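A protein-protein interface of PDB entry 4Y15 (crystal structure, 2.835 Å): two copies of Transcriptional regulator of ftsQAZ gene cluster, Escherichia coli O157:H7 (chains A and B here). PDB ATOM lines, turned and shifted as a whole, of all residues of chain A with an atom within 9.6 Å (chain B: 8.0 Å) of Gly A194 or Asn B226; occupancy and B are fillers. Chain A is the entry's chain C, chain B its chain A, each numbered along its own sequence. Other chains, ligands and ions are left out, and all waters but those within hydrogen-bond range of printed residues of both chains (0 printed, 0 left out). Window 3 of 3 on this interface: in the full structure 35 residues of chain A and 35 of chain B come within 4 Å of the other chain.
Thr A191 touches Thr B228, and with the chains exchanged Thr A228 touches Thr B191. Of the 13 pairs that touch across the chains among the printed residues, 2 have their exchanged pair printed and touching as well.
Hydrophobic or aromatic side chains of chain B within 4 Å of the printed part of chain A: Phe B52, Pro B225 and Tyr B233. Of the 19 printed residues of chain A, 7 touch a printed residue of chain B. Hydrophobic or aromatic side chains of chain A within 4 Å of the printed part of chain B: Ala A192 and Ala A231.
Among the printed residues, pairs that only touch across the chains: Arg A189 with Phe B52 (3.8 Å), Thr A191 with Thr B228 (3.4 Å), Ala A192 with Phe B52 (3.4 Å), Ala A192 with Gln B229 (3.2 Å), Ala A192 with Cys B232 (3.6 Å), Ala A192 with Tyr B233 (3.8 Å), Glu A193 with Pro B225 (3.998 Å), Thr A228 with Thr B191 (3.6 Å) and Ala A231 with Cys B232 (3.4 Å).
The side-chain amide oxygen of Gln B215 sits at hydrogen-bond distance from the side-chain hydroxyl of Thr B191, at 3.5 Å. O of Pro B225 is in hydrogen-bond range of NE2 of Gln B219, at 3.4 Å. The backbone NH of Thr B228 is in hydrogen-bond range of the side-chain amide oxygen of Asn B226, at 2.9 Å. The backbone NH (N) of Gln B229 lies within hydrogen-bond range of the side-chain amide oxygen (OD1) of Asn B226, 3.3 Å away. The backbone carbonyl oxygen of Thr B228 lies within hydrogen-bond range of the side-chain sulfur of Cys B232 (3.4 Å). O of Ile A187 lies within hydrogen-bond range of OG1 of Thr A191, 2.8 Å away.
Printed residues of chain B within 4 Å of Gly A194: Asn B226. Asn B226 touches one residue of chain A. Printed residues of chain A within 4 Å of Cys B232: Ala A192 (3.6 Å) and Ala A231 (3.4 Å). Printed residues of chain B within 4 Å of Ala A231: Cys B232 (3.4 Å). Printed residues of chain B within 4 Å of Thr A228: Thr B191. Printed residues of chain B within 4 Å of Thr A191: Thr B228.
N of Phe B52 lies within hydrogen-bond range of OE2 of Glu A193. The side-chain amide nitrogen (ND2) of Asn B226 sits at hydrogen-bond distance from the backbone carbonyl oxygen (O) of Gly A194, at 2.9 Å. The side-chain amide nitrogen (NE2) of Gln B229 is in hydrogen-bond range of the backbone carbonyl oxygen (O) of Glu A193 (2.7 Å). The side-chain hydroxyl (OH) of Tyr B233 lies within hydrogen-bond range of the side-chain carboxylate (OE1) of Glu A193 (2.9 Å).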
ATOM      1  N   GLU A 186     -19.940  -3.953 -14.763  1.00  0.00           N
ATOM      2  CA  GLU A 186     -21.349  -3.796 -14.439  1.00  0.00           C
ATOM      3  C   GLU A 186     -21.489  -2.952 -13.171  1.00  0.00           C
ATOM      4  O   GLU A 186     -22.378  -2.108 -13.078  1.00  0.00           O
ATOM      5  CB  GLU A 186     -22.027  -5.164 -14.305  1.00  0.00           C
ATOM      6  CG  GLU A 186     -23.522  -5.096 -14.039  1.00  0.00           C
ATOM      7  CD  GLU A 186     -24.167  -6.470 -13.946  1.00  0.00           C
ATOM      8  OE1 GLU A 186     -25.398  -6.538 -13.747  1.00  0.00           O
ATOM      9  OE2 GLU A 186     -23.447  -7.482 -14.093  1.00  0.00           O
ATOM     10  N   ILE A 187     -20.601  -3.177 -12.205  1.00  0.00           N
ATOM     11  CA  ILE A 187     -20.606  -2.406 -10.964  1.00  0.00           C
ATOM     12  C   ILE A 187     -20.283  -0.943 -11.267  1.00  0.00           C
ATOM     13  O   ILE A 187     -20.802  -0.040 -10.611  1.00  0.00           O
ATOM     14  CB  ILE A 187     -19.598  -2.972  -9.928  1.00  0.00           C
ATOM     15  CG1 ILE A 187     -20.069  -4.345  -9.442  1.00  0.00           C
ATOM     16  CG2 ILE A 187     -19.446  -2.028  -8.731  1.00  0.00           C
ATOM     17  CD1 ILE A 187     -19.091  -5.065  -8.531  1.00  0.00           C
ATOM     18  N   LEU A 188     -19.429  -0.711 -12.260  1.00  0.00           N
ATOM     19  CA  LEU A 188     -19.106   0.650 -12.678  1.00  0.00           C
ATOM     20  C   LEU A 188     -20.316   1.354 -13.281  1.00  0.00           C
ATOM     21  O   LEU A 188     -20.564   2.519 -12.969  1.00  0.00           O
ATOM     22  CB  LEU A 188     -17.950   0.660 -13.682  1.00  0.00           C
ATOM     23  CG  LEU A 188     -16.527   0.586 -13.127  1.00  0.00           C
ATOM     24  CD1 LEU A 188     -15.525   0.621 -14.266  1.00  0.00           C
ATOM     25  CD2 LEU A 188     -16.237   1.721 -12.147  1.00  0.00           C
ATOM     26  N   ARG A 189     -21.046   0.669 -14.163  1.00  0.00           N
ATOM     27  CA  ARG A 189     -22.258   1.246 -14.742  1.00  0.00           C
ATOM     28  C   ARG A 189     -23.163   1.729 -13.623  1.00  0.00           C
ATOM     29  O   ARG A 189     -23.819   2.761 -13.739  1.00  0.00           O
ATOM     30  CB  ARG A 189     -23.030   0.241 -15.602  1.00  0.00           C
ATOM     31  CG  ARG A 189     -22.575   0.160 -17.041  1.00  0.00           C
ATOM     32  CD  ARG A 189     -23.513  -0.673 -17.891  1.00  0.00           C
ATOM     33  NE  ARG A 189     -23.498  -2.088 -17.535  1.00  0.00           N
ATOM     34  CZ  ARG A 189     -22.679  -2.999 -18.050  1.00  0.00           C
ATOM     35  NH1 ARG A 189     -21.753  -2.656 -18.938  1.00  0.00           N
ATOM     36  NH2 ARG A 189     -22.774  -4.259 -17.651  1.00  0.00           N
ATOM     37  N   TRP A 190     -23.179   0.970 -12.532  1.00  0.00           N
ATOM     38  CA  TRP A 190     -24.037   1.277 -11.400  1.00  0.00           C
ATOM     39  C   TRP A 190     -23.399   2.343 -10.512  1.00  0.00           C
ATOM     40  O   TRP A 190     -24.105   3.132  -9.888  1.00  0.00           O
ATOM     41  CB  TRP A 190     -24.334   0.006 -10.602  1.00  0.00           C
ATOM     42  CG  TRP A 190     -25.350  -0.871 -11.275  1.00  0.00           C
ATOM     43  CD1 TRP A 190     -25.135  -2.094 -11.843  1.00  0.00           C
ATOM     44  CD2 TRP A 190     -26.736  -0.574 -11.478  1.00  0.00           C
ATOM     45  NE1 TRP A 190     -26.303  -2.582 -12.375  1.00  0.00           N
ATOM     46  CE2 TRP A 190     -27.302  -1.666 -12.164  1.00  0.00           C
ATOM     47  CE3 TRP A 190     -27.555   0.508 -11.143  1.00  0.00           C
ATOM     48  CZ2 TRP A 190     -28.650  -1.709 -12.518  1.00  0.00           C
ATOM     49  CZ3 TRP A 190     -28.892   0.463 -11.495  1.00  0.00           C
ATOM     50  CH2 TRP A 190     -29.425  -0.636 -12.174  1.00  0.00           C
ATOM     51  N   THR A 191     -22.072   2.370 -10.455  1.00  0.00           N
ATOM     52  CA  THR A 191     -21.377   3.419  -9.716  1.00  0.00           C
ATOM     53  C   THR A 191     -21.631   4.769 -10.376  1.00  0.00           C
ATOM     54  O   THR A 191     -21.848   5.774  -9.698  1.00  0.00           O
ATOM     55  CB  THR A 191     -19.855   3.170  -9.649  1.00  0.00           C
ATOM     56  OG1 THR A 191     -19.597   1.930  -8.980  1.00  0.00           O
ATOM     57  CG2 THR A 191     -19.148   4.303  -8.902  1.00  0.00           C
ATOM     58  N   ALA A 192     -21.611   4.779 -11.705  1.00  0.00           N
ATOM     59  CA  ALA A 192     -21.843   5.998 -12.465  1.00  0.00           C
ATOM     60  C   ALA A 192     -23.302   6.435 -12.371  1.00  0.00           C
ATOM     61  O   ALA A 192     -23.626   7.579 -12.674  1.00  0.00           O
ATOM     62  CB  ALA A 192     -21.436   5.806 -13.913  1.00  0.00           C
ATOM     63  N   GLU A 193     -24.179   5.513 -11.982  1.00  0.00           N
ATOM     64  CA  GLU A 193     -25.585   5.837 -11.746  1.00  0.00           C
ATOM     65  C   GLU A 193     -25.809   6.406 -10.342  1.00  0.00           C
ATOM     66  O   GLU A 193     -26.913   6.844 -10.017  1.00  0.00           O
ATOM     67  CB  GLU A 193     -26.462   4.601 -11.960  1.00  0.00           C
ATOM     68  CG  GLU A 193     -26.666   4.226 -13.424  1.00  0.00           C
ATOM     69  CD  GLU A 193     -27.419   5.288 -14.203  1.00  0.00           C
ATOM     70  OE1 GLU A 193     -28.132   6.100 -13.574  1.00  0.00           O
ATOM     71  OE2 GLU A 193     -27.296   5.311 -15.446  1.00  0.00           O
ATOM     72  N   GLY A 194     -24.763   6.392  -9.517  1.00  0.00           N
ATOM     73  CA  GLY A 194     -24.824   6.984  -8.189  1.00  0.00           C
ATOM     74  C   GLY A 194     -25.138   6.009  -7.067  1.00  0.00           C
ATOM     75  O   GLY A 194     -25.596   6.417  -6.000  1.00  0.00           O
ATOM     76  N   LYS A 195     -24.894   4.723  -7.300  1.00  0.00           N
ATOM     77  CA  LYS A 195     -25.227   3.695  -6.319  1.00  0.00           C
ATOM     78  C   LYS A 195     -24.096   3.489  -5.306  1.00  0.00           C
ATOM     79  O   LYS A 195     -22.919   3.494  -5.673  1.00  0.00           O
ATOM     80  CB  LYS A 195     -25.522   2.373  -7.031  1.00  0.00           C
ATOM     81  CG  LYS A 195     -26.562   2.472  -8.145  1.00  0.00           C
ATOM     82  CD  LYS A 195     -27.944   2.872  -7.661  1.00  0.00           C
ATOM     83  CE  LYS A 195     -28.929   2.824  -8.822  1.00  0.00           C
ATOM     84  NZ  LYS A 195     -30.343   3.053  -8.428  1.00  0.00           N
ATOM     85  N   THR A 196     -24.455   3.319  -4.036  1.00  0.00           N
ATOM     86  CA  THR A 196     -23.489   2.969  -2.995  1.00  0.00           C
ATOM     87  C   THR A 196     -23.212   1.470  -3.063  1.00  0.00           C
ATOM     88  O   THR A 196     -24.023   0.719  -3.599  1.00  0.00           O
ATOM     89  CB  THR A 196     -24.006   3.338  -1.585  1.00  0.00           C
ATOM     90  OG1 THR A 196     -24.452   4.700  -1.575  1.00  0.00           O
ATOM     91  CG2 THR A 196     -22.923   3.146  -0.520  1.00  0.00           C
ATOM     92  N   SER A 197     -22.084   1.033  -2.507  1.00  0.00           N
ATOM     93  CA  SER A 197     -21.769  -0.392  -2.439  1.00  0.00           C
ATOM     94  C   SER A 197     -22.921  -1.145  -1.784  1.00  0.00           C
ATOM     95  O   SER A 197     -23.249  -2.266  -2.171  1.00  0.00           O
ATOM     96  CB  SER A 197     -20.471  -0.635  -1.670  1.00  0.00           C
ATOM     97  OG  SER A 197     -19.413   0.147  -2.193  1.00  0.00           O
ATOM     98  N   ALA A 198     -23.519  -0.516  -0.778  1.00  0.00           N
ATOM     99  CA  ALA A 198     -24.675  -1.079  -0.095  1.00  0.00           C
ATOM    100  C   ALA A 198     -25.833  -1.272  -1.073  1.00  0.00           C
ATOM    101  O   ALA A 198     -26.493  -2.311  -1.067  1.00  0.00           O
ATOM    102  CB  ALA A 198     -25.094  -0.176   1.057  1.00  0.00           C
ATOM    103  N   GLU A 199     -26.077  -0.266  -1.908  1.00  0.00           N
ATOM    104  CA  GLU A 199     -27.179  -0.310  -2.867  1.00  0.00           C
ATOM    105  C   GLU A 199     -26.906  -1.267  -4.026  1.00  0.00           C
ATOM    106  O   GLU A 199     -27.813  -1.955  -4.496  1.00  0.00           O
ATOM    107  CB  GLU A 199     -27.464   1.087  -3.424  1.00  0.00           C
ATOM    108  CG  GLU A 199     -27.870   2.114  -2.383  1.00  0.00           C
ATOM    109  CD  GLU A 199     -28.225   3.454  -3.003  1.00  0.00           C
ATOM    110  OE1 GLU A 199     -27.310   4.137  -3.511  1.00  0.00           O
ATOM    111  OE2 GLU A 199     -29.420   3.820  -2.988  1.00  0.00           O
ATOM    112  N   ILE A 200     -25.657  -1.303  -4.482  1.00  0.00           N
ATOM    113  CA  ILE A 200     -25.255  -2.199  -5.564  1.00  0.00           C
ATOM    114  C   ILE A 200     -25.416  -3.652  -5.139  1.00  0.00           C
ATOM    115  O   ILE A 200     -25.817  -4.506  -5.931  1.00  0.00           O
ATOM    116  CB  ILE A 200     -23.786  -1.954  -5.981  1.00  0.00           C
ATOM    117  CG1 ILE A 200     -23.604  -0.521  -6.493  1.00  0.00           C
ATOM    118  CG2 ILE A 200     -23.355  -2.953  -7.057  1.00  0.00           C
ATOM    119  CD1 ILE A 200     -22.160  -0.123  -6.721  1.00  0.00           C
ATOM    120  N   ILE A 203     -29.152  -5.149  -5.569  1.00  0.00           N
ATOM    121  CA  ILE A 203     -29.634  -5.478  -6.911  1.00  0.00           C
ATOM    122  C   ILE A 203     -28.905  -6.673  -7.540  1.00  0.00           C
ATOM    123  O   ILE A 203     -29.534  -7.496  -8.207  1.00  0.00           O
ATOM    124  CB  ILE A 203     -29.547  -4.250  -7.849  1.00  0.00           C
ATOM    125  CG1 ILE A 203     -30.544  -3.185  -7.386  1.00  0.00           C
ATOM    126  CG2 ILE A 203     -29.852  -4.636  -9.298  1.00  0.00           C
ATOM    127  CD1 ILE A 203     -30.363  -1.823  -8.022  1.00  0.00           C
ATOM    128  N   LYS A 227     -13.372   5.602  -6.457  1.00  0.00           N
ATOM    129  CA  LYS A 227     -14.268   5.008  -7.443  1.00  0.00           C
ATOM    130  C   LYS A 227     -14.739   6.041  -8.455  1.00  0.00           C
ATOM    131  O   LYS A 227     -15.174   5.697  -9.554  1.00  0.00           O
ATOM    132  CB  LYS A 227     -15.488   4.388  -6.752  1.00  0.00           C
ATOM    133  CG  LYS A 227     -16.405   5.416  -6.095  1.00  0.00           C
ATOM    134  CD  LYS A 227     -17.535   4.775  -5.306  1.00  0.00           C
ATOM    135  CE  LYS A 227     -18.511   5.838  -4.816  1.00  0.00           C
ATOM    136  NZ  LYS A 227     -19.697   5.266  -4.121  1.00  0.00           N
ATOM    137  N   THR A 228     -14.652   7.312  -8.077  1.00  0.00           N
ATOM    138  CA  THR A 228     -15.124   8.389  -8.934  1.00  0.00           C
ATOM    139  C   THR A 228     -14.237   8.575 -10.168  1.00  0.00           C
ATOM    140  O   THR A 228     -14.753   8.704 -11.278  1.00  0.00           O
ATOM    141  CB  THR A 228     -15.218   9.717  -8.154  1.00  0.00           C
ATOM    142  OG1 THR A 228     -15.955   9.508  -6.944  1.00  0.00           O
ATOM    143  CG2 THR A 228     -15.912  10.784  -8.989  1.00  0.00           C
ATOM    144  N   ALA A 231     -14.750   5.641 -12.709  1.00  0.00           N
ATOM    145  CA  ALA A 231     -16.005   5.691 -13.442  1.00  0.00           C
ATOM    146  C   ALA A 231     -15.947   6.750 -14.538  1.00  0.00           C
ATOM    147  O   ALA A 231     -16.429   6.530 -15.649  1.00  0.00           O
ATOM    148  CB  ALA A 231     -17.161   5.968 -12.497  1.00  0.00           C
ATOM    149  N   PHE B  52     -26.488   5.126 -18.135  1.00  0.00           N
ATOM    150  CA  PHE B  52     -25.623   4.011 -18.507  1.00  0.00           C
ATOM    151  C   PHE B  52     -26.328   2.655 -18.565  1.00  0.00           C
ATOM    152  O   PHE B  52     -25.969   1.807 -19.380  1.00  0.00           O
ATOM    153  CB  PHE B  52     -24.452   3.935 -17.521  1.00  0.00           C
ATOM    154  CG  PHE B  52     -23.576   5.159 -17.526  1.00  0.00           C
ATOM    155  CD1 PHE B  52     -22.602   5.324 -18.496  1.00  0.00           C
ATOM    156  CD2 PHE B  52     -23.746   6.156 -16.578  1.00  0.00           C
ATOM    157  CE1 PHE B  52     -21.798   6.449 -18.508  1.00  0.00           C
ATOM    158  CE2 PHE B  52     -22.948   7.286 -16.589  1.00  0.00           C
ATOM    159  CZ  PHE B  52     -21.973   7.433 -17.556  1.00  0.00           C
ATOM    160  N   LEU B 188     -16.373  20.073 -12.147  1.00  0.00           N
ATOM    161  CA  LEU B 188     -16.642  18.727 -12.640  1.00  0.00           C
ATOM    162  C   LEU B 188     -15.365  18.060 -13.146  1.00  0.00           C
ATOM    163  O   LEU B 188     -15.092  16.908 -12.810  1.00  0.00           O
ATOM    164  CB  LEU B 188     -17.698  18.767 -13.743  1.00  0.00           C
ATOM    165  CG  LEU B 188     -19.157  18.876 -13.283  1.00  0.00           C
ATOM    166  CD1 LEU B 188     -20.085  18.876 -14.483  1.00  0.00           C
ATOM    167  CD2 LEU B 188     -19.550  17.765 -12.312  1.00  0.00           C
ATOM    168  N   THR B 191     -13.545  16.995 -10.213  1.00  0.00           N
ATOM    169  CA  THR B 191     -14.232  15.893  -9.550  1.00  0.00           C
ATOM    170  C   THR B 191     -13.912  14.608 -10.298  1.00  0.00           C
ATOM    171  O   THR B 191     -13.715  13.554  -9.696  1.00  0.00           O
ATOM    172  CB  THR B 191     -15.758  16.110  -9.506  1.00  0.00           C
ATOM    173  OG1 THR B 191     -16.053  17.318  -8.794  1.00  0.00           O
ATOM    174  CG2 THR B 191     -16.460  14.939  -8.825  1.00  0.00           C
ATOM    175  N   GLN B 215     -21.844  22.020  -6.346  1.00  0.00           N
ATOM    176  CA  GLN B 215     -22.034  20.581  -6.453  1.00  0.00           C
ATOM    177  C   GLN B 215     -23.503  20.197  -6.303  1.00  0.00           C
ATOM    178  O   GLN B 215     -24.018  19.372  -7.058  1.00  0.00           O
ATOM    179  CB  GLN B 215     -21.186  19.855  -5.402  1.00  0.00           C
ATOM    180  CG  GLN B 215     -20.612  18.525  -5.865  1.00  0.00           C
ATOM    181  CD  GLN B 215     -19.802  18.652  -7.143  1.00  0.00           C
ATOM    182  OE1 GLN B 215     -18.614  18.978  -7.114  1.00  0.00           O
ATOM    183  NE2 GLN B 215     -20.449  18.405  -8.277  1.00  0.00           N
ATOM    184  N   LYS B 216     -24.174  20.794  -5.323  1.00  0.00           N
ATOM    185  CA  LYS B 216     -25.573  20.479  -5.056  1.00  0.00           C
ATOM    186  C   LYS B 216     -26.482  21.102  -6.109  1.00  0.00           C
ATOM    187  O   LYS B 216     -27.506  20.528  -6.472  1.00  0.00           O
ATOM    188  CB  LYS B 216     -25.985  20.962  -3.663  1.00  0.00           C
ATOM    189  CG  LYS B 216     -25.445  20.120  -2.516  1.00  0.00           C
ATOM    190  CD  LYS B 216     -25.886  20.675  -1.167  1.00  0.00           C
ATOM    191  CE  LYS B 216     -25.360  19.837  -0.014  1.00  0.00           C
ATOM    192  NZ  LYS B 216     -25.716  20.429   1.305  1.00  0.00           N
ATOM    193  N   MET B 218     -25.764  21.611  -9.315  1.00  0.00           N
ATOM    194  CA  MET B 218     -25.719  20.828 -10.544  1.00  0.00           C
ATOM    195  C   MET B 218     -26.602  19.595 -10.395  1.00  0.00           C
ATOM    196  O   MET B 218     -27.260  19.186 -11.347  1.00  0.00           O
ATOM    197  CB  MET B 218     -24.290  20.418 -10.911  1.00  0.00           C
ATOM    198  CG  MET B 218     -23.394  21.578 -11.324  1.00  0.00           C
ATOM    199  SD  MET B 218     -21.719  21.069 -11.771  1.00  0.00           S
ATOM    200  CE  MET B 218     -20.875  21.137 -10.192  1.00  0.00           C
ATOM    201  N   GLN B 219     -26.616  19.016  -9.196  1.00  0.00           N
ATOM    202  CA  GLN B 219     -27.451  17.851  -8.911  1.00  0.00           C
ATOM    203  C   GLN B 219     -28.935  18.204  -8.886  1.00  0.00           C
ATOM    204  O   GLN B 219     -29.781  17.359  -9.174  1.00  0.00           O
ATOM    205  CB  GLN B 219     -27.048  17.210  -7.581  1.00  0.00           C
ATOM    206  CG  GLN B 219     -25.669  16.574  -7.607  1.00  0.00           C
ATOM    207  CD  GLN B 219     -25.086  16.351  -6.225  1.00  0.00           C
ATOM    208  OE1 GLN B 219     -23.880  16.485  -6.023  1.00  0.00           O
ATOM    209  NE2 GLN B 219     -25.940  15.998  -5.271  1.00  0.00           N
ATOM    210  N   ILE B 222     -30.340  18.270 -12.560  1.00  0.00           N
ATOM    211  CA  ILE B 222     -30.185  16.991 -13.262  1.00  0.00           C
ATOM    212  C   ILE B 222     -30.978  15.905 -12.543  1.00  0.00           C
ATOM    213  O   ILE B 222     -31.239  14.840 -13.104  1.00  0.00           O
ATOM    214  CB  ILE B 222     -28.688  16.573 -13.350  1.00  0.00           C
ATOM    215  CG1 ILE B 222     -28.510  15.307 -14.208  1.00  0.00           C
ATOM    216  CG2 ILE B 222     -28.141  16.337 -11.961  1.00  0.00           C
ATOM    217  CD1 ILE B 222     -27.072  14.804 -14.314  1.00  0.00           C
ATOM    218  N   ASN B 223     -31.394  16.199 -11.314  1.00  0.00           N
ATOM    219  CA  ASN B 223     -31.997  15.199 -10.442  1.00  0.00           C
ATOM    220  C   ASN B 223     -31.045  14.024 -10.253  1.00  0.00           C
ATOM    221  O   ASN B 223     -31.355  12.889 -10.619  1.00  0.00           O
ATOM    222  CB  ASN B 223     -33.333  14.720 -11.017  1.00  0.00           C
ATOM    223  CG  ASN B 223     -34.178  13.983  -9.998  1.00  0.00           C
ATOM    224  OD1 ASN B 223     -33.685  13.554  -8.955  1.00  0.00           O
ATOM    225  ND2 ASN B 223     -35.461  13.821 -10.302  1.00  0.00           N
ATOM    226  N   ALA B 224     -29.881  14.317  -9.677  1.00  0.00           N
ATOM    227  CA  ALA B 224     -28.889  13.295  -9.368  1.00  0.00           C
ATOM    228  C   ALA B 224     -28.769  13.102  -7.861  1.00  0.00           C
ATOM    229  O   ALA B 224     -28.948  14.051  -7.098  1.00  0.00           O
ATOM    230  CB  ALA B 224     -27.539  13.671  -9.957  1.00  0.00           C
ATOM    231  N   PRO B 225     -28.467  11.867  -7.425  1.00  0.00           N
ATOM    232  CA  PRO B 225     -28.281  11.595  -5.996  1.00  0.00           C
ATOM    233  C   PRO B 225     -27.052  12.295  -5.429  1.00  0.00           C
ATOM    234  O   PRO B 225     -27.120  12.953  -4.391  1.00  0.00           O
ATOM    235  CB  PRO B 225     -28.102  10.074  -5.941  1.00  0.00           C
ATOM    236  CG  PRO B 225     -27.655   9.687  -7.306  1.00  0.00           C
ATOM    237  CD  PRO B 225     -28.293  10.656  -8.245  1.00  0.00           C
ATOM    238  N   ASN B 226     -25.936  12.141  -6.134  1.00  0.00           N
ATOM    239  CA  ASN B 226     -24.631  12.564  -5.646  1.00  0.00           C
ATOM    240  C   ASN B 226     -23.771  13.147  -6.760  1.00  0.00           C
ATOM    241  O   ASN B 226     -24.201  13.231  -7.908  1.00  0.00           O
ATOM    242  CB  ASN B 226     -23.920  11.376  -5.010  1.00  0.00           C
ATOM    243  CG  ASN B 226     -23.899  10.169  -5.920  1.00  0.00           C
ATOM    244  OD1 ASN B 226     -23.247  10.178  -6.961  1.00  0.00           O
ATOM    245  ND2 ASN B 226     -24.635   9.130  -5.546  1.00  0.00           N
ATOM    246  N   LYS B 227     -22.553  13.546  -6.414  1.00  0.00           N
ATOM    247  CA  LYS B 227     -21.652  14.178  -7.371  1.00  0.00           C
ATOM    248  C   LYS B 227     -21.076  13.173  -8.372  1.00  0.00           C
ATOM    249  O   LYS B 227     -20.577  13.567  -9.426  1.00  0.00           O
ATOM    250  CB  LYS B 227     -20.524  14.913  -6.634  1.00  0.00           C
ATOM    251  CG  LYS B 227     -19.568  14.028  -5.846  1.00  0.00           C
ATOM    252  CD  LYS B 227     -18.581  14.876  -5.049  1.00  0.00           C
ATOM    253  CE  LYS B 227     -17.514  14.029  -4.367  1.00  0.00           C
ATOM    254  NZ  LYS B 227     -16.490  14.865  -3.675  1.00  0.00           N
ATOM    255  N   THR B 228     -21.145  11.882  -8.053  1.00  0.00           N
ATOM    256  CA  THR B 228     -20.576  10.857  -8.929  1.00  0.00           C
ATOM    257  C   THR B 228     -21.345  10.747 -10.243  1.00  0.00           C
ATOM    258  O   THR B 228     -20.740  10.705 -11.314  1.00  0.00           O
ATOM    259  CB  THR B 228     -20.562   9.467  -8.255  1.00  0.00           C
ATOM    260  OG1 THR B 228     -19.963   9.561  -6.957  1.00  0.00           O
ATOM    261  CG2 THR B 228     -19.789   8.462  -9.100  1.00  0.00           C
ATOM    262  N   GLN B 229     -22.672  10.701 -10.165  1.00  0.00           N
ATOM    263  CA  GLN B 229     -23.493  10.556 -11.362  1.00  0.00           C
ATOM    264  C   GLN B 229     -23.363  11.776 -12.261  1.00  0.00           C
ATOM    265  O   GLN B 229     -23.375  11.662 -13.487  1.00  0.00           O
ATOM    266  CB  GLN B 229     -24.962  10.331 -10.994  1.00  0.00           C
ATOM    267  CG  GLN B 229     -25.819   9.851 -12.161  1.00  0.00           C
ATOM    268  CD  GLN B 229     -27.303   9.970 -11.891  1.00  0.00           C
ATOM    269  OE1 GLN B 229     -27.877  11.057 -11.962  1.00  0.00           O
ATOM    270  NE2 GLN B 229     -27.937   8.846 -11.578  1.00  0.00           N
ATOM    271  N   VAL B 230     -23.236  12.943 -11.642  1.00  0.00           N
ATOM    272  CA  VAL B 230     -23.165  14.195 -12.379  1.00  0.00           C
ATOM    273  C   VAL B 230     -21.866  14.256 -13.176  1.00  0.00           C
ATOM    274  O   VAL B 230     -21.853  14.671 -14.336  1.00  0.00           O
ATOM    275  CB  VAL B 230     -23.265  15.403 -11.423  1.00  0.00           C
ATOM    276  CG1 VAL B 230     -23.243  16.717 -12.194  1.00  0.00           C
ATOM    277  CG2 VAL B 230     -24.528  15.305 -10.588  1.00  0.00           C
ATOM    278  N   ALA B 231     -20.774  13.837 -12.547  1.00  0.00           N
ATOM    279  CA  ALA B 231     -19.464  13.841 -13.187  1.00  0.00           C
ATOM    280  C   ALA B 231     -19.392  12.850 -14.346  1.00  0.00           C
ATOM    281  O   ALA B 231     -18.829  13.152 -15.399  1.00  0.00           O
ATOM    282  CB  ALA B 231     -18.384  13.530 -12.162  1.00  0.00           C
ATOM    283  N   CYS B 232     -19.961  11.665 -14.145  1.00  0.00           N
ATOM    284  CA  CYS B 232     -19.900  10.598 -15.140  1.00  0.00           C
ATOM    285  C   CYS B 232     -20.748  10.904 -16.369  1.00  0.00           C
ATOM    286  O   CYS B 232     -20.348  10.615 -17.496  1.00  0.00           O
ATOM    287  CB  CYS B 232     -20.347   9.276 -14.521  1.00  0.00           C
ATOM    288  SG  CYS B 232     -19.138   8.561 -13.388  1.00  0.00           S
ATOM    289  N   TYR B 233     -21.925  11.480 -16.145  1.00  0.00           N
ATOM    290  CA  TYR B 233     -22.799  11.881 -17.239  1.00  0.00           C
ATOM    291  C   TYR B 233     -22.104  12.951 -18.074  1.00  0.00           C
ATOM    292  O   TYR B 233     -22.175  12.946 -19.300  1.00  0.00           O
ATOM    293  CB  TYR B 233     -24.126  12.419 -16.705  1.00  0.00           C
ATOM    294  CG  TYR B 233     -25.125  11.348 -16.331  1.00  0.00           C
ATOM    295  CD1 TYR B 233     -26.489  11.573 -16.441  1.00  0.00           C
ATOM    296  CD2 TYR B 233     -24.701  10.119 -15.845  1.00  0.00           C
ATOM    297  CE1 TYR B 233     -27.403  10.600 -16.089  1.00  0.00           C
ATOM    298  CE2 TYR B 233     -25.605   9.141 -15.489  1.00  0.00           C
ATOM    299  CZ  TYR B 233     -26.954   9.387 -15.610  1.00  0.00           C
ATOM    300  OH  TYR B 233     -27.854   8.411 -15.254  1.00  0.00           O
